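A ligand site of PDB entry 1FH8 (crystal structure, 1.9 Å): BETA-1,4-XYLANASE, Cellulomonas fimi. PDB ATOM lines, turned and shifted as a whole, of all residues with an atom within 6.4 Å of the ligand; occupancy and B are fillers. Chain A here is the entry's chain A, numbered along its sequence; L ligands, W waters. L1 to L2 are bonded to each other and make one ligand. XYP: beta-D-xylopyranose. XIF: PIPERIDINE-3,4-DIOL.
A nitrogen (N1) of XIF L2 is in salt-bridge range of the side-chain carboxylate (OE1) of Glu 233, 2.6 Å away.
An oxygen (O2) of XYP L1 lies within hydrogen-bond range of the side-chain carboxylate of Glu 43 (2.8 Å).
A ring nitrogen (NE2) of His 80 sits at hydrogen-bond distance from an oxygen (O3) of XIF L2.
The indole nitrogen (NE1) of Trp 273 lies within hydrogen-bond range of an oxygen (O2) of XYP L1, 2.8 Å away.
NZ of Lys 47 is in hydrogen-bond range of O3 of XIF L2, at 2.9 Å.
A nitrogen (N1) of XIF L2 lies within salt-bridge range of the side-chain carboxylate (OE2) of Glu 127, 3.1 Å away.
OE1 of Gln 203 sits at hydrogen-bond distance from N1 of XIF L2.
The side-chain amide nitrogen (ND2) of Asn 44 is in hydrogen-bond range of an oxygen (O3) of XYP L1 (3.1 Å).
NE2 of Gln 87 lies within hydrogen-bond range of O5 of XYP L1 (3.1 Å).
N of Glu 233 sits close to O of Gln 203 (2.9 Å).
The side-chain amide nitrogen of Asn 169 sits at hydrogen-bond distance from the side-chain carboxylate of Glu 233, 3.0 Å away.
The side-chain carboxylate of Glu 127 is in hydrogen-bond range of the side-chain amide nitrogen of Gln 203, at 2.8 Å.
N of Glu 127 sits at hydrogen-bond distance from O of Asn 169 (2.9 Å).
The side-chain amide oxygen (OD1) of Asn 126 is in hydrogen-bond range of the side-chain amide nitrogen (NE2) of Gln 203, at 3.1 Å.
The side-chain amide nitrogen of Gln 203 sits close to the side-chain amide nitrogen of Asn 169 (3.2 Å).
The indole nitrogen of Trp 84 sits close to the side-chain amide nitrogen of Asn 126 (3.2 Å).
The side-chain amide nitrogen (ND2) of Asn 169 sits at hydrogen-bond distance from the side-chain amide oxygen (OD1) of Asn 126, at 3.0 Å.
CH2 of Trp 84 touches O3 of XIF L2, 3.4 Å away.
ND2 of Asn 126 touches C2 of XIF L2 (3.8 Å).
NE2 of His 205 touches N1 of XIF L2, at 3.7 Å.
CB of Trp 281 touches O2 of XYP L1, 3.2 Å away.
Hydrophobic or aromatic side chains within 4 Å of the ligand: His 80, Trp 84, Trp 273 and Trp 281.
Within 4 Å of the ligand: Glu 43, Asn 44, Lys 47, His 80, Trp 84, Gln 87, Asn 126, Glu 127, Gln 203, His 205, Glu 233, Trp 273 and Trp 281.
The nearest printed residue that does not touch the ligand is Thr 81 (5.4 Å).
Water W1 lies within hydrogen-bond range of OG of Ser 86 (2.8 Å) and NE2 of Gln 87 (2.9 Å).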
ATOM      1  N   GLU A  43       5.436  14.468   3.723  1.00  0.00           N
ATOM      2  CA  GLU A  43       4.141  14.968   4.154  1.00  0.00           C
ATOM      3  C   GLU A  43       3.557  14.061   5.219  1.00  0.00           C
ATOM      4  O   GLU A  43       2.821  14.519   6.107  1.00  0.00           O
ATOM      5  CB  GLU A  43       3.173  15.080   2.957  1.00  0.00           C
ATOM      6  CG  GLU A  43       1.748  15.430   3.357  1.00  0.00           C
ATOM      7  CD  GLU A  43       0.798  15.572   2.181  1.00  0.00           C
ATOM      8  OE1 GLU A  43       0.958  14.850   1.180  1.00  0.00           O
ATOM      9  OE2 GLU A  43      -0.122  16.408   2.274  1.00  0.00           O
ATOM     10  N   ASN A  44       3.899  12.781   5.164  1.00  0.00           N
ATOM     11  CA  ASN A  44       3.370  11.824   6.127  1.00  0.00           C
ATOM     12  C   ASN A  44       4.309  10.655   6.422  1.00  0.00           C
ATOM     13  O   ASN A  44       4.229  10.042   7.473  1.00  0.00           O
ATOM     14  CB  ASN A  44       2.042  11.236   5.629  1.00  0.00           C
ATOM     15  CG  ASN A  44       0.877  12.203   5.781  1.00  0.00           C
ATOM     16  OD1 ASN A  44       0.550  12.616   6.890  1.00  0.00           O
ATOM     17  ND2 ASN A  44       0.259  12.558   4.673  1.00  0.00           N
ATOM     18  N   LYS A  47       6.108  10.407   9.988  1.00  0.00           N
ATOM     19  CA  LYS A  47       5.354  10.601  11.216  1.00  0.00           C
ATOM     20  C   LYS A  47       5.317   9.292  11.994  1.00  0.00           C
ATOM     21  O   LYS A  47       5.643   8.237  11.471  1.00  0.00           O
ATOM     22  CB  LYS A  47       3.928  11.073  10.884  1.00  0.00           C
ATOM     23  CG  LYS A  47       3.888  12.490  10.299  1.00  0.00           C
ATOM     24  CD  LYS A  47       2.487  12.872   9.813  1.00  0.00           C
ATOM     25  CE  LYS A  47       2.470  14.280   9.227  1.00  0.00           C
ATOM     26  NZ  LYS A  47       1.146  14.628   8.620  1.00  0.00           N
ATOM     27  N   HIS A  80      10.028  15.565   9.378  1.00  0.00           N
ATOM     28  CA  HIS A  80       8.761  15.917   9.976  1.00  0.00           C
ATOM     29  C   HIS A  80       8.046  14.628  10.312  1.00  0.00           C
ATOM     30  O   HIS A  80       7.716  13.901   9.394  1.00  0.00           O
ATOM     31  CB  HIS A  80       7.994  16.689   8.902  1.00  0.00           C
ATOM     32  CG  HIS A  80       6.626  17.128   9.307  1.00  0.00           C
ATOM     33  ND1 HIS A  80       6.400  18.231  10.109  1.00  0.00           N
ATOM     34  CD2 HIS A  80       5.404  16.634   8.995  1.00  0.00           C
ATOM     35  CE1 HIS A  80       5.102  18.389  10.288  1.00  0.00           C
ATOM     36  NE2 HIS A  80       4.473  17.430   9.620  1.00  0.00           N
ATOM     37  N   THR A  81       7.786  14.305  11.585  1.00  0.00           N
ATOM     38  CA  THR A  81       8.110  15.075  12.784  1.00  0.00           C
ATOM     39  C   THR A  81       8.215  14.049  13.918  1.00  0.00           C
ATOM     40  O   THR A  81       7.610  12.994  13.877  1.00  0.00           O
ATOM     41  CB  THR A  81       7.014  16.181  13.092  1.00  0.00           C
ATOM     42  OG1 THR A  81       7.242  16.752  14.389  1.00  0.00           O
ATOM     43  CG2 THR A  81       5.617  15.604  13.029  1.00  0.00           C
ATOM     44  N   TRP A  84       4.295  14.482  17.996  1.00  0.00           N
ATOM     45  CA  TRP A  84       3.110  15.232  17.617  1.00  0.00           C
ATOM     46  C   TRP A  84       1.885  14.530  18.199  1.00  0.00           C
ATOM     47  O   TRP A  84       1.826  13.302  18.234  1.00  0.00           O
ATOM     48  CB  TRP A  84       3.022  15.284  16.082  1.00  0.00           C
ATOM     49  CG  TRP A  84       1.897  16.105  15.525  1.00  0.00           C
ATOM     50  CD1 TRP A  84       1.355  17.235  16.050  1.00  0.00           C
ATOM     51  CD2 TRP A  84       1.229  15.886  14.267  1.00  0.00           C
ATOM     52  NE1 TRP A  84       0.397  17.749  15.206  1.00  0.00           N
ATOM     53  CE2 TRP A  84       0.300  16.944  14.099  1.00  0.00           C
ATOM     54  CE3 TRP A  84       1.329  14.909  13.270  1.00  0.00           C
ATOM     55  CZ2 TRP A  84      -0.527  17.046  12.972  1.00  0.00           C
ATOM     56  CZ3 TRP A  84       0.514  15.010  12.137  1.00  0.00           C
ATOM     57  CH2 TRP A  84      -0.409  16.069  12.000  1.00  0.00           C
ATOM     58  N   SER A  86      -1.053  14.404  16.957  1.00  0.00           N
ATOM     59  CA  SER A  86      -1.879  13.814  15.900  1.00  0.00           C
ATOM     60  C   SER A  86      -1.169  12.672  15.175  1.00  0.00           C
ATOM     61  O   SER A  86       0.060  12.561  15.206  1.00  0.00           O
ATOM     62  CB  SER A  86      -2.293  14.897  14.905  1.00  0.00           C
ATOM     63  OG  SER A  86      -3.359  14.451  14.110  1.00  0.00           O
ATOM     64  N   GLN A  87      -1.947  11.824  14.520  1.00  0.00           N
ATOM     65  CA  GLN A  87      -1.437  10.654  13.800  1.00  0.00           C
ATOM     66  C   GLN A  87      -0.504   9.826  14.675  1.00  0.00           C
ATOM     67  O   GLN A  87       0.555   9.361  14.234  1.00  0.00           O
ATOM     68  CB  GLN A  87      -0.741  11.077  12.499  1.00  0.00           C
ATOM     69  CG  GLN A  87      -1.736  11.520  11.432  1.00  0.00           C
ATOM     70  CD  GLN A  87      -1.071  11.949  10.147  1.00  0.00           C
ATOM     71  OE1 GLN A  87      -0.548  11.131   9.387  1.00  0.00           O
ATOM     72  NE2 GLN A  87      -1.096  13.254   9.887  1.00  0.00           N
ATOM     73  N   ASN A 126       6.061  19.075  17.361  1.00  0.00           N
ATOM     74  CA  ASN A 126       5.149  19.798  16.498  1.00  0.00           C
ATOM     75  C   ASN A 126       3.834  20.131  17.180  1.00  0.00           C
ATOM     76  O   ASN A 126       3.230  19.275  17.819  1.00  0.00           O
ATOM     77  CB  ASN A 126       4.883  18.970  15.238  1.00  0.00           C
ATOM     78  CG  ASN A 126       4.002  19.687  14.237  1.00  0.00           C
ATOM     79  OD1 ASN A 126       4.272  20.828  13.877  1.00  0.00           O
ATOM     80  ND2 ASN A 126       2.953  19.013  13.774  1.00  0.00           N
ATOM     81  N   GLU A 127       3.415  21.382  17.029  1.00  0.00           N
ATOM     82  CA  GLU A 127       2.142  21.884  17.562  1.00  0.00           C
ATOM     83  C   GLU A 127       1.908  21.671  19.049  1.00  0.00           C
ATOM     84  O   GLU A 127       0.859  21.171  19.474  1.00  0.00           O
ATOM     85  CB  GLU A 127       0.999  21.277  16.732  1.00  0.00           C
ATOM     86  CG  GLU A 127       1.051  21.738  15.269  1.00  0.00           C
ATOM     87  CD  GLU A 127       0.145  20.954  14.327  1.00  0.00           C
ATOM     88  OE1 GLU A 127      -0.879  20.410  14.787  1.00  0.00           O
ATOM     89  OE2 GLU A 127       0.446  20.902  13.109  1.00  0.00           O
ATOM     90  N   ASN A 169       8.037  23.234  15.699  1.00  0.00           N
ATOM     91  CA  ASN A 169       7.184  23.750  14.641  1.00  0.00           C
ATOM     92  C   ASN A 169       5.772  23.960  15.172  1.00  0.00           C
ATOM     93  O   ASN A 169       5.347  23.295  16.108  1.00  0.00           O
ATOM     94  CB  ASN A 169       7.209  22.717  13.509  1.00  0.00           C
ATOM     95  CG  ASN A 169       6.568  23.214  12.229  1.00  0.00           C
ATOM     96  OD1 ASN A 169       6.981  24.218  11.651  1.00  0.00           O
ATOM     97  ND2 ASN A 169       5.563  22.475  11.743  1.00  0.00           N
ATOM     98  N   TYR A 171       1.627  26.216  14.168  1.00  0.00           N
ATOM     99  CA  TYR A 171       0.839  27.070  13.289  1.00  0.00           C
ATOM    100  C   TYR A 171       0.146  28.168  14.086  1.00  0.00           C
ATOM    101  O   TYR A 171       0.088  28.109  15.328  1.00  0.00           O
ATOM    102  CB  TYR A 171      -0.185  26.212  12.518  1.00  0.00           C
ATOM    103  CG  TYR A 171      -1.252  25.604  13.385  1.00  0.00           C
ATOM    104  CD1 TYR A 171      -2.442  26.291  13.654  1.00  0.00           C
ATOM    105  CD2 TYR A 171      -1.086  24.345  13.960  1.00  0.00           C
ATOM    106  CE1 TYR A 171      -3.434  25.738  14.466  1.00  0.00           C
ATOM    107  CE2 TYR A 171      -2.068  23.782  14.776  1.00  0.00           C
ATOM    108  CZ  TYR A 171      -3.235  24.485  15.028  1.00  0.00           C
ATOM    109  OH  TYR A 171      -4.208  23.925  15.830  1.00  0.00           O
ATOM    110  N   GLN A 203       4.581  27.122  10.291  1.00  0.00           N
ATOM    111  CA  GLN A 203       3.786  26.401   9.303  1.00  0.00           C
ATOM    112  C   GLN A 203       3.198  27.288   8.196  1.00  0.00           C
ATOM    113  O   GLN A 203       3.338  26.975   7.015  1.00  0.00           O
ATOM    114  CB  GLN A 203       2.685  25.621  10.024  1.00  0.00           C
ATOM    115  CG  GLN A 203       3.195  24.356  10.712  1.00  0.00           C
ATOM    116  CD  GLN A 203       2.083  23.536  11.340  1.00  0.00           C
ATOM    117  OE1 GLN A 203       0.932  23.588  10.893  1.00  0.00           O
ATOM    118  NE2 GLN A 203       2.410  22.765  12.365  1.00  0.00           N
ATOM    119  N   HIS A 205      -0.163  28.065   7.399  1.00  0.00           N
ATOM    120  CA  HIS A 205      -1.314  27.549   6.671  1.00  0.00           C
ATOM    121  C   HIS A 205      -2.257  28.743   6.785  1.00  0.00           C
ATOM    122  O   HIS A 205      -3.059  28.846   7.712  1.00  0.00           O
ATOM    123  CB  HIS A 205      -1.884  26.312   7.367  1.00  0.00           C
ATOM    124  CG  HIS A 205      -1.059  25.080   7.196  1.00  0.00           C
ATOM    125  ND1 HIS A 205      -0.855  24.476   5.966  1.00  0.00           N
ATOM    126  CD2 HIS A 205      -0.370  24.332   8.097  1.00  0.00           C
ATOM    127  CE1 HIS A 205      -0.078  23.425   6.125  1.00  0.00           C
ATOM    128  NE2 HIS A 205       0.236  23.315   7.402  1.00  0.00           N
ATOM    129  N   GLU A 233       5.215  24.902   6.179  1.00  0.00           N
ATOM    130  CA  GLU A 233       4.069  24.269   5.534  1.00  0.00           C
ATOM    131  C   GLU A 233       3.154  25.269   4.856  1.00  0.00           C
ATOM    132  O   GLU A 233       1.931  25.230   5.013  1.00  0.00           O
ATOM    133  CB  GLU A 233       3.296  23.475   6.574  1.00  0.00           C
ATOM    134  CG  GLU A 233       4.168  22.539   7.398  1.00  0.00           C
ATOM    135  CD  GLU A 233       3.422  21.870   8.533  1.00  0.00           C
ATOM    136  OE1 GLU A 233       2.172  21.860   8.507  1.00  0.00           O
ATOM    137  OE2 GLU A 233       4.093  21.344   9.446  1.00  0.00           O
ATOM    138  N   TRP A 273       3.362  23.281   1.509  1.00  0.00           N
ATOM    139  CA  TRP A 273       2.796  21.977   1.865  1.00  0.00           C
ATOM    140  C   TRP A 273       2.140  21.249   0.702  1.00  0.00           C
ATOM    141  O   TRP A 273       0.935  21.013   0.707  1.00  0.00           O
ATOM    142  CB  TRP A 273       1.804  22.151   3.028  1.00  0.00           C
ATOM    143  CG  TRP A 273       1.691  20.902   3.863  1.00  0.00           C
ATOM    144  CD1 TRP A 273       0.586  20.115   4.038  1.00  0.00           C
ATOM    145  CD2 TRP A 273       2.753  20.272   4.591  1.00  0.00           C
ATOM    146  NE1 TRP A 273       0.895  19.031   4.811  1.00  0.00           N
ATOM    147  CE2 TRP A 273       2.220  19.098   5.162  1.00  0.00           C
ATOM    148  CE3 TRP A 273       4.104  20.580   4.794  1.00  0.00           C
ATOM    149  CZ2 TRP A 273       2.989  18.228   5.945  1.00  0.00           C
ATOM    150  CZ3 TRP A 273       4.880  19.717   5.575  1.00  0.00           C
ATOM    151  CH2 TRP A 273       4.320  18.555   6.138  1.00  0.00           C
ATOM    152  N   TYR A 279      -3.703  17.345  -4.992  1.00  0.00           N
ATOM    153  CA  TYR A 279      -3.442  16.502  -3.820  1.00  0.00           C
ATOM    154  C   TYR A 279      -3.427  17.216  -2.463  1.00  0.00           C
ATOM    155  O   TYR A 279      -3.301  16.581  -1.419  1.00  0.00           O
ATOM    156  CB  TYR A 279      -2.125  15.753  -4.048  1.00  0.00           C
ATOM    157  CG  TYR A 279      -2.163  14.863  -5.266  1.00  0.00           C
ATOM    158  CD1 TYR A 279      -1.113  14.832  -6.177  1.00  0.00           C
ATOM    159  CD2 TYR A 279      -3.278  14.061  -5.515  1.00  0.00           C
ATOM    160  CE1 TYR A 279      -1.167  14.017  -7.327  1.00  0.00           C
ATOM    161  CE2 TYR A 279      -3.354  13.244  -6.644  1.00  0.00           C
ATOM    162  CZ  TYR A 279      -2.292  13.232  -7.545  1.00  0.00           C
ATOM    163  OH  TYR A 279      -2.363  12.427  -8.663  1.00  0.00           O
ATOM    164  N   SER A 280      -3.561  18.543  -2.479  1.00  0.00           N
ATOM    165  CA  SER A 280      -3.553  19.334  -1.258  1.00  0.00           C
ATOM    166  C   SER A 280      -4.442  18.774  -0.147  1.00  0.00           C
ATOM    167  O   SER A 280      -5.548  18.291  -0.408  1.00  0.00           O
ATOM    168  CB  SER A 280      -3.981  20.779  -1.553  1.00  0.00           C
ATOM    169  OG  SER A 280      -4.122  21.503  -0.336  1.00  0.00           O
ATOM    170  N   TRP A 281      -3.965  18.877   1.081  1.00  0.00           N
ATOM    171  CA  TRP A 281      -4.708  18.383   2.242  1.00  0.00           C
ATOM    172  C   TRP A 281      -5.901  19.255   2.609  1.00  0.00           C
ATOM    173  O   TRP A 281      -6.802  18.800   3.313  1.00  0.00           O
ATOM    174  CB  TRP A 281      -3.797  18.292   3.469  1.00  0.00           C
ATOM    175  CG  TRP A 281      -3.459  19.628   4.059  1.00  0.00           C
ATOM    176  CD1 TRP A 281      -2.859  20.676   3.431  1.00  0.00           C
ATOM    177  CD2 TRP A 281      -3.702  20.053   5.412  1.00  0.00           C
ATOM    178  NE1 TRP A 281      -2.707  21.730   4.299  1.00  0.00           N
ATOM    179  CE2 TRP A 281      -3.221  21.379   5.523  1.00  0.00           C
ATOM    180  CE3 TRP A 281      -4.281  19.444   6.541  1.00  0.00           C
ATOM    181  CZ2 TRP A 281      -3.293  22.101   6.720  1.00  0.00           C
ATOM    182  CZ3 TRP A 281      -4.350  20.175   7.727  1.00  0.00           C
ATOM    183  CH2 TRP A 281      -3.870  21.493   7.804  1.00  0.00           C
ATOM    184  N   VAL A 285      -9.973  18.784   4.969  1.00  0.00           N
ATOM    185  CA  VAL A 285      -9.963  19.304   6.331  1.00  0.00           C
ATOM    186  C   VAL A 285     -10.807  20.559   6.459  1.00  0.00           C
ATOM    187  O   VAL A 285     -11.449  20.782   7.487  1.00  0.00           O
ATOM    188  CB  VAL A 285      -8.530  19.616   6.788  1.00  0.00           C
ATOM    189  CG1 VAL A 285      -8.535  20.242   8.168  1.00  0.00           C
ATOM    190  CG2 VAL A 285      -7.711  18.341   6.778  1.00  0.00           C
HETATM  191  C1  XYP L   1      -1.326  16.761   7.166  1.00  0.00           C
HETATM  192  C2  XYP L   1      -1.213  16.085   5.783  1.00  0.00           C
HETATM  193  C3  XYP L   1      -2.437  15.211   5.499  1.00  0.00           C
HETATM  194  C4  XYP L   1      -2.751  14.293   6.700  1.00  0.00           C
HETATM  195  C5  XYP L   1      -2.793  15.095   8.001  1.00  0.00           C
HETATM  196  O2  XYP L   1      -1.085  17.077   4.772  1.00  0.00           O
HETATM  197  O3  XYP L   1      -2.177  14.413   4.359  1.00  0.00           O
HETATM  198  O4  XYP L   1      -3.979  13.615   6.494  1.00  0.00           O
HETATM  199  O5  XYP L   1      -1.555  15.789   8.194  1.00  0.00           O
HETATM  200  N1  XIF L   2       0.387  20.705   9.987  1.00  0.00           N
HETATM  201  C2  XIF L   2       1.005  19.432  10.480  1.00  0.00           C
HETATM  202  C3  XIF L   2       1.143  18.489   9.239  1.00  0.00           C
HETATM  203  O3  XIF L   2       1.717  17.243   9.602  1.00  0.00           O
HETATM  204  C4  XIF L   2      -0.246  18.302   8.589  1.00  0.00           C
HETATM  205  O4  XIF L   2      -0.092  17.443   7.470  1.00  0.00           O
HETATM  206  C5  XIF L   2      -0.842  19.677   8.197  1.00  0.00           C
HETATM  207  C6  XIF L   2      -0.944  20.486   9.448  1.00  0.00           C
HETATM  208  O   HOH W   1      -3.192  14.539  11.340  1.00  0.00           O
HETATM  209  O   HOH W   2      -4.441  11.680   8.888  1.00  0.00           O
HETATM  210  O   HOH W   3      -4.630  14.162   2.449  1.00  0.00           O
